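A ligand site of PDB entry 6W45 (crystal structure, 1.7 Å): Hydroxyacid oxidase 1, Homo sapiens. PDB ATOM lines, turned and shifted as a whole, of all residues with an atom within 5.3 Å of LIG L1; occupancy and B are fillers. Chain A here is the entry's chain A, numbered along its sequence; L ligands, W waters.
Water W2 lies within hydrogen-bond range of O9 of LIG L1 (2.8 Å), ND2 of Asn 40 (2.9 Å), NH1 of Arg 315 (3.1 Å) and O of Gly 261 (3.5 Å).
Water W1 lies within hydrogen-bond range of OD2 of Asp 291 (2.8 Å) and O3 of LIG L1 (3.0 Å).
An oxygen (O3) of LIG L1 sits at hydrogen-bond distance from the backbone carbonyl oxygen of Ala 79, 2.6 Å away.
An oxygen (O2) of LIG L1 is in hydrogen-bond range of the side-chain hydroxyl of Ser 108, at 2.7 Å.
An oxygen (O1) of LIG L1 sits at hydrogen-bond distance from the side-chain hydroxyl (OG1) of Thr 158 (2.7 Å).
The guanidinium group (NH2) of Arg 295 is in salt-bridge range of an oxygen (O9) of LIG L1.
The side-chain carboxylate (OD2) of Asp 291 is in hydrogen-bond range of an oxygen (O4) of LIG L1, 2.8 Å away.
The side-chain amino group (NZ) of Lys 236 lies within hydrogen-bond range of an oxygen (O1) of LIG L1, 2.8 Å away.
The side-chain amide oxygen (OE1) of Gln 130 sits at hydrogen-bond distance from a nitrogen (N2) of LIG L1 (2.8 Å).
O7 of LIG L1 sits at hydrogen-bond distance from N of Gly 314, 2.9 Å away.
An oxygen (O9) of LIG L1 lies within hydrogen-bond range of the backbone NH (N) of Gly 293, at 2.9 Å.
The backbone NH (N) of Arg 315 sits at hydrogen-bond distance from an oxygen (O8) of LIG L1.
NH1 of Arg 315 lies within salt-bridge range of O8 of LIG L1, 3.0 Å away.
N of Ala 81 sits at hydrogen-bond distance from N3 of LIG L1 (3.1 Å).
The side-chain hydroxyl (OG) of Ser 258 lies within hydrogen-bond range of an oxygen (O4) of LIG L1, at 3.3 Å.
An oxygen (O6) of LIG L1 sits close to the backbone NH (N) of Gly 292 (3.5 Å).
N1 of LIG L1 lies within hydrogen-bond range of NE2 of His 260, at 3.5 Å.
An oxygen (O3) of LG2 L2 lies within hydrogen-bond range of a ring nitrogen (NE2) of His 260 (2.7 Å).
OH of Tyr 132 is in hydrogen-bond range of O2 of LG2 L2.
Residues that only touch LIG L1: Tyr 27 (3.6 Å), Thr 80 (3.6 Å), Trp 110 (3.7 Å), Tyr 132 (3.9 Å), Gly 261 (3.5 Å), Arg 263 (3.5 Å) and Val 313 (3.8 Å).
Within 4 Å of LIG L1: Tyr 27, Ala 79, Thr 80, Ala 81, Ser 108, Trp 110, Gln 130, Tyr 132, Thr 158, Lys 236, Ser 258, His 260, Gly 261, Arg 263, Asp 291, Gly 292, Gly 293, Arg 295, Val 313, Gly 314 and Arg 315.
Along chain A the residues within 4 Å of LIG L1 span positions 27 to 315.
The nearest printed residue that does not touch LIG L1 is Pro 316 (4.03 Å).
A nitrogen (N2) of LIG L1 lies close to an oxygen (O2) of LG2 L2 (3.2 Å).
OG of Ser 108 lies within hydrogen-bond range of N of Trp 110, at 2.7 Å.
The side-chain amide nitrogen (NE2) of Gln 130 is in hydrogen-bond range of the side-chain hydroxyl (OG1) of Thr 158, 3.1 Å away.
The side-chain carboxylate (OD1) of Asp 291 sits at hydrogen-bond distance from the side-chain hydroxyl (OG) of Ser 258 (2.6 Å).
The side-chain amide oxygen (OE1) of Gln 130 lies within hydrogen-bond range of the backbone NH (N) of Ser 109 (2.9 Å).
The guanidinium group (NH2) of Arg 315 lies within hydrogen-bond range of the backbone carbonyl oxygen (O) of Gly 261 (2.8 Å).
N of His 260 is in hydrogen-bond range of OG of Ser 258, 2.9 Å away.
The backbone carbonyl oxygen (O) of Tyr 27 is in hydrogen-bond range of the guanidinium group (NH1) of Arg 263, 3.4 Å away.
The backbone NH (N) of Gly 78 is in hydrogen-bond range of the backbone carbonyl oxygen (O) of Val 313 (2.8 Å).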
ATOM      1  N   TYR A  26     -22.782 -25.796  12.413  1.00  0.00           N
ATOM      2  CA  TYR A  26     -23.592 -25.823  11.167  1.00  0.00           C
ATOM      3  C   TYR A  26     -23.008 -24.796  10.181  1.00  0.00           C
ATOM      4  O   TYR A  26     -22.785 -25.102   8.966  1.00  0.00           O
ATOM      5  CB  TYR A  26     -25.069 -25.527  11.402  1.00  0.00           C
ATOM      6  CG  TYR A  26     -25.814 -25.289  10.110  1.00  0.00           C
ATOM      7  CD1 TYR A  26     -26.039 -26.355   9.258  1.00  0.00           C
ATOM      8  CD2 TYR A  26     -26.204 -24.034   9.696  1.00  0.00           C
ATOM      9  CE1 TYR A  26     -26.653 -26.156   8.033  1.00  0.00           C
ATOM     10  CE2 TYR A  26     -26.831 -23.815   8.479  1.00  0.00           C
ATOM     11  CZ  TYR A  26     -27.016 -24.900   7.634  1.00  0.00           C
ATOM     12  OH  TYR A  26     -27.584 -24.710   6.429  1.00  0.00           O
ATOM     13  N   TYR A  27     -22.727 -23.594  10.662  1.00  0.00           N
ATOM     14  CA  TYR A  27     -22.221 -22.504   9.795  1.00  0.00           C
ATOM     15  C   TYR A  27     -20.779 -22.785   9.390  1.00  0.00           C
ATOM     16  O   TYR A  27     -20.415 -22.518   8.220  1.00  0.00           O
ATOM     17  CB  TYR A  27     -22.334 -21.154  10.528  1.00  0.00           C
ATOM     18  CG  TYR A  27     -23.728 -20.602  10.679  1.00  0.00           C
ATOM     19  CD1 TYR A  27     -24.602 -20.458   9.622  1.00  0.00           C
ATOM     20  CD2 TYR A  27     -24.105 -20.071  11.922  1.00  0.00           C
ATOM     21  CE1 TYR A  27     -25.844 -19.851   9.776  1.00  0.00           C
ATOM     22  CE2 TYR A  27     -25.338 -19.464  12.079  1.00  0.00           C
ATOM     23  CZ  TYR A  27     -26.208 -19.349  11.011  1.00  0.00           C
ATOM     24  OH  TYR A  27     -27.391 -18.678  11.120  1.00  0.00           O
ATOM     25  N   ASN A  40      -9.593 -23.705   0.584  1.00  0.00           N
ATOM     26  CA  ASN A  40     -10.150 -22.421   0.084  1.00  0.00           C
ATOM     27  C   ASN A  40      -9.378 -21.270   0.708  1.00  0.00           C
ATOM     28  O   ASN A  40      -9.114 -20.264   0.032  1.00  0.00           O
ATOM     29  CB  ASN A  40     -11.634 -22.268   0.413  1.00  0.00           C
ATOM     30  CG  ASN A  40     -12.567 -22.888  -0.619  1.00  0.00           C
ATOM     31  OD1 ASN A  40     -12.096 -23.343  -1.686  1.00  0.00           O
ATOM     32  ND2 ASN A  40     -13.853 -22.930  -0.288  1.00  0.00           N
ATOM     33  N   GLY A  78     -22.745 -12.931  -0.245  1.00  0.00           N
ATOM     34  CA  GLY A  78     -23.250 -14.173  -0.868  1.00  0.00           C
ATOM     35  C   GLY A  78     -24.431 -14.780  -0.101  1.00  0.00           C
ATOM     36  O   GLY A  78     -24.588 -14.520   1.095  1.00  0.00           O
ATOM     37  N   ALA A  79     -25.173 -15.658  -0.757  1.00  0.00           N
ATOM     38  CA  ALA A  79     -26.353 -16.347  -0.177  1.00  0.00           C
ATOM     39  C   ALA A  79     -25.930 -17.260   0.965  1.00  0.00           C
ATOM     40  O   ALA A  79     -25.110 -18.178   0.759  1.00  0.00           O
ATOM     41  CB  ALA A  79     -27.099 -17.109  -1.258  1.00  0.00           C
ATOM     42  N   THR A  80     -26.514 -17.093   2.160  1.00  0.00           N
ATOM     43  CA  THR A  80     -26.306 -18.061   3.264  1.00  0.00           C
ATOM     44  C   THR A  80     -27.682 -18.288   3.895  1.00  0.00           C
ATOM     45  O   THR A  80     -28.344 -17.289   4.210  1.00  0.00           O
ATOM     46  CB  THR A  80     -25.283 -17.640   4.327  1.00  0.00           C
ATOM     47  OG1 THR A  80     -25.548 -16.292   4.711  1.00  0.00           O
ATOM     48  CG2 THR A  80     -23.866 -17.677   3.816  1.00  0.00           C
ATOM     49  N   ALA A  81     -28.130 -19.534   3.919  1.00  0.00           N
ATOM     50  CA  ALA A  81     -29.468 -19.905   4.439  1.00  0.00           C
ATOM     51  C   ALA A  81     -29.613 -19.465   5.901  1.00  0.00           C
ATOM     52  O   ALA A  81     -28.627 -19.525   6.658  1.00  0.00           O
ATOM     53  CB  ALA A  81     -29.615 -21.387   4.321  1.00  0.00           C
ATOM     54  N   MET A 106     -26.916 -10.940  -2.199  1.00  0.00           N
ATOM     55  CA  MET A 106     -27.502 -12.145  -2.827  1.00  0.00           C
ATOM     56  C   MET A 106     -28.352 -12.842  -1.779  1.00  0.00           C
ATOM     57  O   MET A 106     -27.790 -13.305  -0.761  1.00  0.00           O
ATOM     58  CB  MET A 106     -26.395 -13.083  -3.322  1.00  0.00           C
ATOM     59  CG  MET A 106     -26.900 -14.186  -4.204  1.00  0.00           C
ATOM     60  SD  MET A 106     -25.749 -15.588  -4.322  1.00  0.00           S
ATOM     61  CE  MET A 106     -24.282 -14.769  -4.917  1.00  0.00           C
ATOM     62  N   SER A 108     -30.579 -15.713  -0.229  1.00  0.00           N
ATOM     63  CA  SER A 108     -30.679 -17.186  -0.276  1.00  0.00           C
ATOM     64  C   SER A 108     -32.093 -17.605  -0.654  1.00  0.00           C
ATOM     65  O   SER A 108     -33.054 -16.930  -0.242  1.00  0.00           O
ATOM     66  CB  SER A 108     -30.364 -17.829   1.060  1.00  0.00           C
ATOM     67  OG  SER A 108     -30.761 -19.203   1.048  1.00  0.00           O
ATOM     68  N   SER A 109     -32.206 -18.723  -1.352  1.00  0.00           N
ATOM     69  CA  SER A 109     -33.491 -19.434  -1.583  1.00  0.00           C
ATOM     70  C   SER A 109     -34.079 -20.003  -0.290  1.00  0.00           C
ATOM     71  O   SER A 109     -35.312 -20.321  -0.277  1.00  0.00           O
ATOM     72  CB  SER A 109     -33.309 -20.550  -2.618  1.00  0.00           C
ATOM     73  OG  SER A 109     -34.009 -20.196  -3.792  1.00  0.00           O
ATOM     74  N   TRP A 110     -33.286 -20.120   0.761  1.00  0.00           N
ATOM     75  CA  TRP A 110     -33.698 -20.743   2.048  1.00  0.00           C
ATOM     76  C   TRP A 110     -33.660 -19.683   3.158  1.00  0.00           C
ATOM     77  O   TRP A 110     -33.086 -19.978   4.247  1.00  0.00           O
ATOM     78  CB  TRP A 110     -32.793 -21.920   2.390  1.00  0.00           C
ATOM     79  CG  TRP A 110     -32.797 -22.991   1.359  1.00  0.00           C
ATOM     80  CD1 TRP A 110     -31.802 -23.297   0.460  1.00  0.00           C
ATOM     81  CD2 TRP A 110     -33.867 -23.915   1.102  1.00  0.00           C
ATOM     82  NE1 TRP A 110     -32.186 -24.339  -0.323  1.00  0.00           N
ATOM     83  CE2 TRP A 110     -33.441 -24.752   0.049  1.00  0.00           C
ATOM     84  CE3 TRP A 110     -35.123 -24.127   1.698  1.00  0.00           C
ATOM     85  CZ2 TRP A 110     -34.258 -25.790  -0.425  1.00  0.00           C
ATOM     86  CZ3 TRP A 110     -35.918 -25.154   1.218  1.00  0.00           C
ATOM     87  CH2 TRP A 110     -35.484 -25.961   0.168  1.00  0.00           C
ATOM     88  N   GLN A 130     -30.774 -15.596  -5.216  1.00  0.00           N
ATOM     89  CA  GLN A 130     -30.219 -16.931  -5.477  1.00  0.00           C
ATOM     90  C   GLN A 130     -31.392 -17.906  -5.532  1.00  0.00           C
ATOM     91  O   GLN A 130     -32.211 -17.897  -4.609  1.00  0.00           O
ATOM     92  CB  GLN A 130     -29.174 -17.300  -4.434  1.00  0.00           C
ATOM     93  CG  GLN A 130     -28.713 -18.732  -4.576  1.00  0.00           C
ATOM     94  CD  GLN A 130     -29.553 -19.776  -3.879  1.00  0.00           C
ATOM     95  OE1 GLN A 130     -29.828 -19.680  -2.685  1.00  0.00           O
ATOM     96  NE2 GLN A 130     -29.867 -20.849  -4.597  1.00  0.00           N
ATOM     97  N   TYR A 132     -32.721 -22.063  -6.787  1.00  0.00           N
ATOM     98  CA  TYR A 132     -32.599 -23.443  -7.263  1.00  0.00           C
ATOM     99  C   TYR A 132     -33.717 -23.677  -8.287  1.00  0.00           C
ATOM    100  O   TYR A 132     -34.819 -23.107  -8.114  1.00  0.00           O
ATOM    101  CB  TYR A 132     -32.734 -24.403  -6.087  1.00  0.00           C
ATOM    102  CG  TYR A 132     -31.508 -24.450  -5.207  1.00  0.00           C
ATOM    103  CD1 TYR A 132     -30.375 -25.099  -5.663  1.00  0.00           C
ATOM    104  CD2 TYR A 132     -31.459 -23.866  -3.954  1.00  0.00           C
ATOM    105  CE1 TYR A 132     -29.227 -25.143  -4.902  1.00  0.00           C
ATOM    106  CE2 TYR A 132     -30.328 -23.943  -3.156  1.00  0.00           C
ATOM    107  CZ  TYR A 132     -29.208 -24.580  -3.645  1.00  0.00           C
ATOM    108  OH  TYR A 132     -28.040 -24.622  -2.930  1.00  0.00           O
ATOM    109  N   THR A 158     -28.023 -21.611  -8.550  1.00  0.00           N
ATOM    110  CA  THR A 158     -27.032 -22.545  -7.964  1.00  0.00           C
ATOM    111  C   THR A 158     -27.123 -23.881  -8.698  1.00  0.00           C
ATOM    112  O   THR A 158     -28.258 -24.463  -8.779  1.00  0.00           O
ATOM    113  CB  THR A 158     -27.216 -22.659  -6.453  1.00  0.00           C
ATOM    114  OG1 THR A 158     -27.148 -21.346  -5.899  1.00  0.00           O
ATOM    115  CG2 THR A 158     -26.170 -23.600  -5.887  1.00  0.00           C
ATOM    116  N   LYS A 236     -23.977 -20.266 -10.614  1.00  0.00           N
ATOM    117  CA  LYS A 236     -23.198 -20.321  -9.359  1.00  0.00           C
ATOM    118  C   LYS A 236     -22.823 -21.763  -9.048  1.00  0.00           C
ATOM    119  O   LYS A 236     -23.724 -22.599  -8.856  1.00  0.00           O
ATOM    120  CB  LYS A 236     -24.051 -19.710  -8.242  1.00  0.00           C
ATOM    121  CG  LYS A 236     -23.465 -19.836  -6.846  1.00  0.00           C
ATOM    122  CD  LYS A 236     -24.341 -19.131  -5.822  1.00  0.00           C
ATOM    123  CE  LYS A 236     -23.768 -19.108  -4.422  1.00  0.00           C
ATOM    124  NZ  LYS A 236     -23.876 -20.410  -3.726  1.00  0.00           N
ATOM    125  N   SER A 258     -17.322 -21.150  -7.617  1.00  0.00           N
ATOM    126  CA  SER A 258     -17.787 -21.467  -6.256  1.00  0.00           C
ATOM    127  C   SER A 258     -17.727 -22.984  -6.087  1.00  0.00           C
ATOM    128  O   SER A 258     -18.095 -23.720  -7.026  1.00  0.00           O
ATOM    129  CB  SER A 258     -19.181 -20.939  -6.004  1.00  0.00           C
ATOM    130  OG  SER A 258     -19.628 -21.305  -4.673  1.00  0.00           O
ATOM    131  N   HIS A 260     -19.297 -23.844  -3.214  1.00  0.00           N
ATOM    132  CA  HIS A 260     -20.450 -23.816  -2.259  1.00  0.00           C
ATOM    133  C   HIS A 260     -19.860 -23.742  -0.852  1.00  0.00           C
ATOM    134  O   HIS A 260     -20.377 -24.444   0.071  1.00  0.00           O
ATOM    135  CB  HIS A 260     -21.313 -25.067  -2.445  1.00  0.00           C
ATOM    136  CG  HIS A 260     -22.740 -24.875  -2.052  1.00  0.00           C
ATOM    137  ND1 HIS A 260     -23.790 -24.931  -2.981  1.00  0.00           N
ATOM    138  CD2 HIS A 260     -23.301 -24.699  -0.822  1.00  0.00           C
ATOM    139  CE1 HIS A 260     -24.943 -24.781  -2.327  1.00  0.00           C
ATOM    140  NE2 HIS A 260     -24.670 -24.585  -0.982  1.00  0.00           N
ATOM    141  N   GLY A 261     -18.798 -22.985  -0.687  1.00  0.00           N
ATOM    142  CA  GLY A 261     -18.110 -22.845   0.641  1.00  0.00           C
ATOM    143  C   GLY A 261     -17.592 -24.211   1.138  1.00  0.00           C
ATOM    144  O   GLY A 261     -17.508 -24.456   2.362  1.00  0.00           O
ATOM    145  N   ARG A 263     -18.935 -27.129   0.980  1.00  0.00           N
ATOM    146  CA  ARG A 263     -20.025 -27.860   1.669  1.00  0.00           C
ATOM    147  C   ARG A 263     -20.654 -28.914   0.742  1.00  0.00           C
ATOM    148  O   ARG A 263     -21.584 -29.621   1.200  1.00  0.00           O
ATOM    149  CB  ARG A 263     -21.086 -26.859   2.135  1.00  0.00           C
ATOM    150  CG  ARG A 263     -20.567 -25.923   3.207  1.00  0.00           C
ATOM    151  CD  ARG A 263     -21.584 -24.854   3.501  1.00  0.00           C
ATOM    152  NE  ARG A 263     -22.743 -25.291   4.291  1.00  0.00           N
ATOM    153  CZ  ARG A 263     -22.821 -25.275   5.626  1.00  0.00           C
ATOM    154  NH1 ARG A 263     -21.778 -24.991   6.370  1.00  0.00           N
ATOM    155  NH2 ARG A 263     -23.972 -25.593   6.218  1.00  0.00           N
ATOM    156  N   ASP A 291     -16.305 -16.925  -4.993  1.00  0.00           N
ATOM    157  CA  ASP A 291     -16.510 -17.029  -3.527  1.00  0.00           C
ATOM    158  C   ASP A 291     -15.730 -18.245  -3.029  1.00  0.00           C
ATOM    159  O   ASP A 291     -15.253 -19.040  -3.844  1.00  0.00           O
ATOM    160  CB  ASP A 291     -17.980 -17.050  -3.101  1.00  0.00           C
ATOM    161  CG  ASP A 291     -18.811 -18.251  -3.493  1.00  0.00           C
ATOM    162  OD1 ASP A 291     -18.225 -19.337  -3.685  1.00  0.00           O
ATOM    163  OD2 ASP A 291     -20.062 -18.106  -3.587  1.00  0.00           O
ATOM    164  N   GLY A 292     -15.617 -18.363  -1.711  1.00  0.00           N
ATOM    165  CA  GLY A 292     -14.923 -19.487  -1.105  1.00  0.00           C
ATOM    166  C   GLY A 292     -13.626 -19.011  -0.473  1.00  0.00           C
ATOM    167  O   GLY A 292     -12.625 -18.874  -1.156  1.00  0.00           O
ATOM    168  N   GLY A 293     -13.589 -18.810   0.833  1.00  0.00           N
ATOM    169  CA  GLY A 293     -12.325 -18.547   1.500  1.00  0.00           C
ATOM    170  C   GLY A 293     -11.933 -17.076   1.567  1.00  0.00           C
ATOM    171  O   GLY A 293     -10.869 -16.802   2.069  1.00  0.00           O
ATOM    172  N   VAL A 294     -12.731 -16.130   1.083  1.00  0.00           N
ATOM    173  CA  VAL A 294     -12.379 -14.690   1.151  1.00  0.00           C
ATOM    174  C   VAL A 294     -12.523 -14.210   2.605  1.00  0.00           C
ATOM    175  O   VAL A 294     -13.639 -14.274   3.104  1.00  0.00           O
ATOM    176  CB  VAL A 294     -13.233 -13.850   0.221  1.00  0.00           C
ATOM    177  CG1 VAL A 294     -12.872 -12.411   0.342  1.00  0.00           C
ATOM    178  CG2 VAL A 294     -13.045 -14.319  -1.202  1.00  0.00           C
ATOM    179  N   ARG A 295     -11.421 -13.810   3.203  1.00  0.00           N
ATOM    180  CA  ARG A 295     -11.366 -13.373   4.635  1.00  0.00           C
ATOM    181  C   ARG A 295     -10.638 -12.044   4.777  1.00  0.00           C
ATOM    182  O   ARG A 295     -10.798 -11.430   5.855  1.00  0.00           O
ATOM    183  CB  ARG A 295     -10.660 -14.435   5.472  1.00  0.00           C
ATOM    184  CG  ARG A 295     -11.305 -15.814   5.428  1.00  0.00           C
ATOM    185  CD  ARG A 295     -12.700 -15.909   5.989  1.00  0.00           C
ATOM    186  NE  ARG A 295     -13.292 -17.234   5.887  1.00  0.00           N
ATOM    187  CZ  ARG A 295     -14.156 -17.665   4.939  1.00  0.00           C
ATOM    188  NH1 ARG A 295     -14.588 -16.840   3.995  1.00  0.00           N
ATOM    189  NH2 ARG A 295     -14.618 -18.892   4.981  1.00  0.00           N
ATOM    190  N   PHE A 312     -17.661 -12.648  -3.530  1.00  0.00           N
ATOM    191  CA  PHE A 312     -18.767 -12.770  -2.541  1.00  0.00           C
ATOM    192  C   PHE A 312     -18.232 -13.393  -1.281  1.00  0.00           C
ATOM    193  O   PHE A 312     -17.359 -14.275  -1.351  1.00  0.00           O
ATOM    194  CB  PHE A 312     -19.903 -13.573  -3.124  1.00  0.00           C
ATOM    195  CG  PHE A 312     -20.598 -12.900  -4.262  1.00  0.00           C
ATOM    196  CD1 PHE A 312     -20.042 -12.914  -5.537  1.00  0.00           C
ATOM    197  CD2 PHE A 312     -21.767 -12.192  -4.077  1.00  0.00           C
ATOM    198  CE1 PHE A 312     -20.653 -12.251  -6.587  1.00  0.00           C
ATOM    199  CE2 PHE A 312     -22.383 -11.548  -5.150  1.00  0.00           C
ATOM    200  CZ  PHE A 312     -21.842 -11.594  -6.398  1.00  0.00           C
ATOM    201  N   VAL A 313     -18.823 -12.994  -0.170  1.00  0.00           N
ATOM    202  CA  VAL A 313     -18.455 -13.584   1.149  1.00  0.00           C
ATOM    203  C   VAL A 313     -19.720 -14.226   1.734  1.00  0.00           C
ATOM    204  O   VAL A 313     -20.791 -13.605   1.659  1.00  0.00           O
ATOM    205  CB  VAL A 313     -17.847 -12.563   2.132  1.00  0.00           C
ATOM    206  CG1 VAL A 313     -16.396 -12.252   1.715  1.00  0.00           C
ATOM    207  CG2 VAL A 313     -18.633 -11.279   2.229  1.00  0.00           C
ATOM    208  N   GLY A 314     -19.541 -15.423   2.270  1.00  0.00           N
ATOM    209  CA  GLY A 314     -20.581 -16.193   2.968  1.00  0.00           C
ATOM    210  C   GLY A 314     -20.435 -16.095   4.445  1.00  0.00           C
ATOM    211  O   GLY A 314     -21.080 -15.249   5.084  1.00  0.00           O
ATOM    212  N   ARG A 315     -19.617 -16.953   5.018  1.00  0.00           N
ATOM    213  CA  ARG A 315     -19.493 -17.116   6.480  1.00  0.00           C
ATOM    214  C   ARG A 315     -19.209 -15.783   7.172  1.00  0.00           C
ATOM    215  O   ARG A 315     -19.774 -15.552   8.271  1.00  0.00           O
ATOM    216  CB  ARG A 315     -18.507 -18.192   6.863  1.00  0.00           C
ATOM    217  CG  ARG A 315     -18.956 -19.583   6.471  1.00  0.00           C
ATOM    218  CD  ARG A 315     -17.931 -20.614   6.763  1.00  0.00           C
ATOM    219  NE  ARG A 315     -18.306 -21.951   6.358  1.00  0.00           N
ATOM    220  CZ  ARG A 315     -18.034 -22.488   5.174  1.00  0.00           C
ATOM    221  NH1 ARG A 315     -17.473 -21.733   4.231  1.00  0.00           N
ATOM    222  NH2 ARG A 315     -18.327 -23.750   4.953  1.00  0.00           N
ATOM    223  N   PRO A 316     -18.324 -14.895   6.662  1.00  0.00           N
ATOM    224  CA  PRO A 316     -17.976 -13.682   7.404  1.00  0.00           C
ATOM    225  C   PRO A 316     -19.239 -12.864   7.778  1.00  0.00           C
ATOM    226  O   PRO A 316     -19.260 -12.306   8.883  1.00  0.00           O
ATOM    227  CB  PRO A 316     -17.077 -12.906   6.452  1.00  0.00           C
ATOM    228  CG  PRO A 316     -16.345 -14.067   5.725  1.00  0.00           C
ATOM    229  CD  PRO A 316     -17.472 -15.033   5.454  1.00  0.00           C
HETATM  230  N1  LIG L   1     -25.407 -21.230  -1.333  1.00  0.00           N
HETATM  231  C1  LIG L   1     -26.571 -21.100  -1.982  1.00  0.00           C
HETATM  232  O1  LIG L   1     -26.580 -20.981  -3.257  1.00  0.00           O
HETATM  233  N2  LIG L   1     -27.772 -21.023  -1.290  1.00  0.00           N
HETATM  234  C2  LIG L   1     -27.794 -21.155   0.039  1.00  0.00           C
HETATM  235  O2  LIG L   1     -28.874 -21.124   0.693  1.00  0.00           O
HETATM  236  C3  LIG L   1     -26.554 -21.316   0.764  1.00  0.00           C
HETATM  237  N3  LIG L   1     -26.496 -21.468   2.150  1.00  0.00           N
HETATM  238  C4  LIG L   1     -25.345 -21.536   2.757  1.00  0.00           C
HETATM  239  C5  LIG L   1     -25.340 -21.600   4.147  1.00  0.00           C
HETATM  240  C6  LIG L   1     -24.161 -21.670   4.811  1.00  0.00           C
HETATM  241  C7  LIG L   1     -24.090 -21.756   6.326  1.00  0.00           C
HETATM  242  C8  LIG L   1     -22.892 -21.594   4.120  1.00  0.00           C
HETATM  243  C9  LIG L   1     -21.613 -21.595   4.890  1.00  0.00           C
HETATM  244  C10 LIG L   1     -22.851 -21.470   2.753  1.00  0.00           C
HETATM  245  C11 LIG L   1     -24.073 -21.470   2.056  1.00  0.00           C
HETATM  246  N4  LIG L   1     -24.130 -21.358   0.668  1.00  0.00           N
HETATM  247  C12 LIG L   1     -25.324 -21.290   0.021  1.00  0.00           C
HETATM  248  C13 LIG L   1     -22.893 -21.220  -0.119  1.00  0.00           C
HETATM  249  C14 LIG L   1     -22.559 -19.736  -0.165  1.00  0.00           C
HETATM  250  O3  LIG L   1     -23.414 -19.016  -1.080  1.00  0.00           O
HETATM  251  C15 LIG L   1     -21.107 -19.425  -0.583  1.00  0.00           C
HETATM  252  O4  LIG L   1     -20.856 -20.150  -1.841  1.00  0.00           O
HETATM  253  C16 LIG L   1     -20.054 -19.821   0.378  1.00  0.00           C
HETATM  254  O5  LIG L   1     -20.481 -19.436   1.728  1.00  0.00           O
HETATM  255  C17 LIG L   1     -18.757 -19.030   0.104  1.00  0.00           C
HETATM  256  O6  LIG L   1     -17.678 -19.428   0.896  1.00  0.00           O
HETATM  257  P1  LIG L   1     -17.251 -18.617   2.270  1.00  0.00           P
HETATM  258  O7  LIG L   1     -17.261 -17.136   2.018  1.00  0.00           O
HETATM  259  O8  LIG L   1     -18.321 -19.051   3.315  1.00  0.00           O
HETATM  260  O9  LIG L   1     -15.928 -19.188   2.554  1.00  0.00           O
HETATM  261  C1  LG2 L   2     -30.021 -27.506   5.872  1.00  0.00           C
HETATM  262  C2  LG2 L   2     -31.392 -26.956   5.577  1.00  0.00           C
HETATM  263  C3  LG2 L   2     -32.450 -27.243   6.457  1.00  0.00           C
HETATM  264  C4  LG2 L   2     -31.642 -26.170   4.456  1.00  0.00           C
HETATM  265  C5  LG2 L   2     -30.575 -25.799   3.480  1.00  0.00           C
HETATM  266  C6  LG2 L   2     -29.504 -24.999   3.843  1.00  0.00           C
HETATM  267  C7  LG2 L   2     -28.568 -24.604   2.902  1.00  0.00           C
HETATM  268  C8  LG2 L   2     -28.659 -25.016   1.586  1.00  0.00           C
HETATM  269  C9  LG2 L   2     -27.624 -24.536   0.608  1.00  0.00           C
HETATM  270  C10 LG2 L   2     -29.703 -25.856   1.246  1.00  0.00           C
HETATM  271  C11 LG2 L   2     -30.665 -26.241   2.162  1.00  0.00           C
HETATM  272  C12 LG2 L   2     -29.749 -29.288   7.628  1.00  0.00           C
HETATM  273  C13 LG2 L   2     -29.591 -28.294   8.709  1.00  0.00           C
HETATM  274  C14 LG2 L   2     -29.768 -25.568  11.096  1.00  0.00           C
HETATM  275  C15 LG2 L   2     -29.208 -25.530  12.361  1.00  0.00           C
HETATM  276  C16 LG2 L   2     -28.469 -26.596  12.796  1.00  0.00           C
HETATM  277  C17 LG2 L   2     -28.257 -27.720  12.013  1.00  0.00           C
HETATM  278 CL1  LG2 L   2     -27.773 -26.546  14.387  1.00  0.00          CL
HETATM  279  C18 LG2 L   2     -28.837 -27.739  10.744  1.00  0.00           C
HETATM  280  C19 LG2 L   2     -29.600 -26.673  10.274  1.00  0.00           C
HETATM  281  C20 LG2 L   2     -30.084 -27.058   8.978  1.00  0.00           C
HETATM  282  N1  LG2 L   2     -28.825 -28.712   9.772  1.00  0.00           N
HETATM  283  O1  LG2 L   2     -29.590 -30.484   7.874  1.00  0.00           O
HETATM  284  N2  LG2 L   2     -30.039 -28.887   6.348  1.00  0.00           N
HETATM  285  C21 LG2 L   2     -30.435 -29.903   5.380  1.00  0.00           C
HETATM  286  C22 LG2 L   2     -32.920 -25.688   4.208  1.00  0.00           C
HETATM  287  C23 LG2 L   2     -33.926 -26.003   5.087  1.00  0.00           C
HETATM  288  F1  LG2 L   2     -35.194 -25.570   4.799  1.00  0.00           F
HETATM  289  C24 LG2 L   2     -33.728 -26.762   6.210  1.00  0.00           C
HETATM  290 CL2  LG2 L   2     -29.792 -26.558  -0.338  1.00  0.00          CL
HETATM  291  O2  LG2 L   2     -27.956 -24.124  -0.476  1.00  0.00           O
HETATM  292  O3  LG2 L   2     -26.414 -24.616   1.033  1.00  0.00           O
HETATM  293  O   HOH W   1     -22.267 -16.672  -2.544  1.00  0.00           O
HETATM  294  O   HOH W   2     -15.209 -21.852   2.094  1.00  0.00           O
HETATM  295  O   HOH W   3     -15.796 -16.205   0.067  1.00  0.00           O
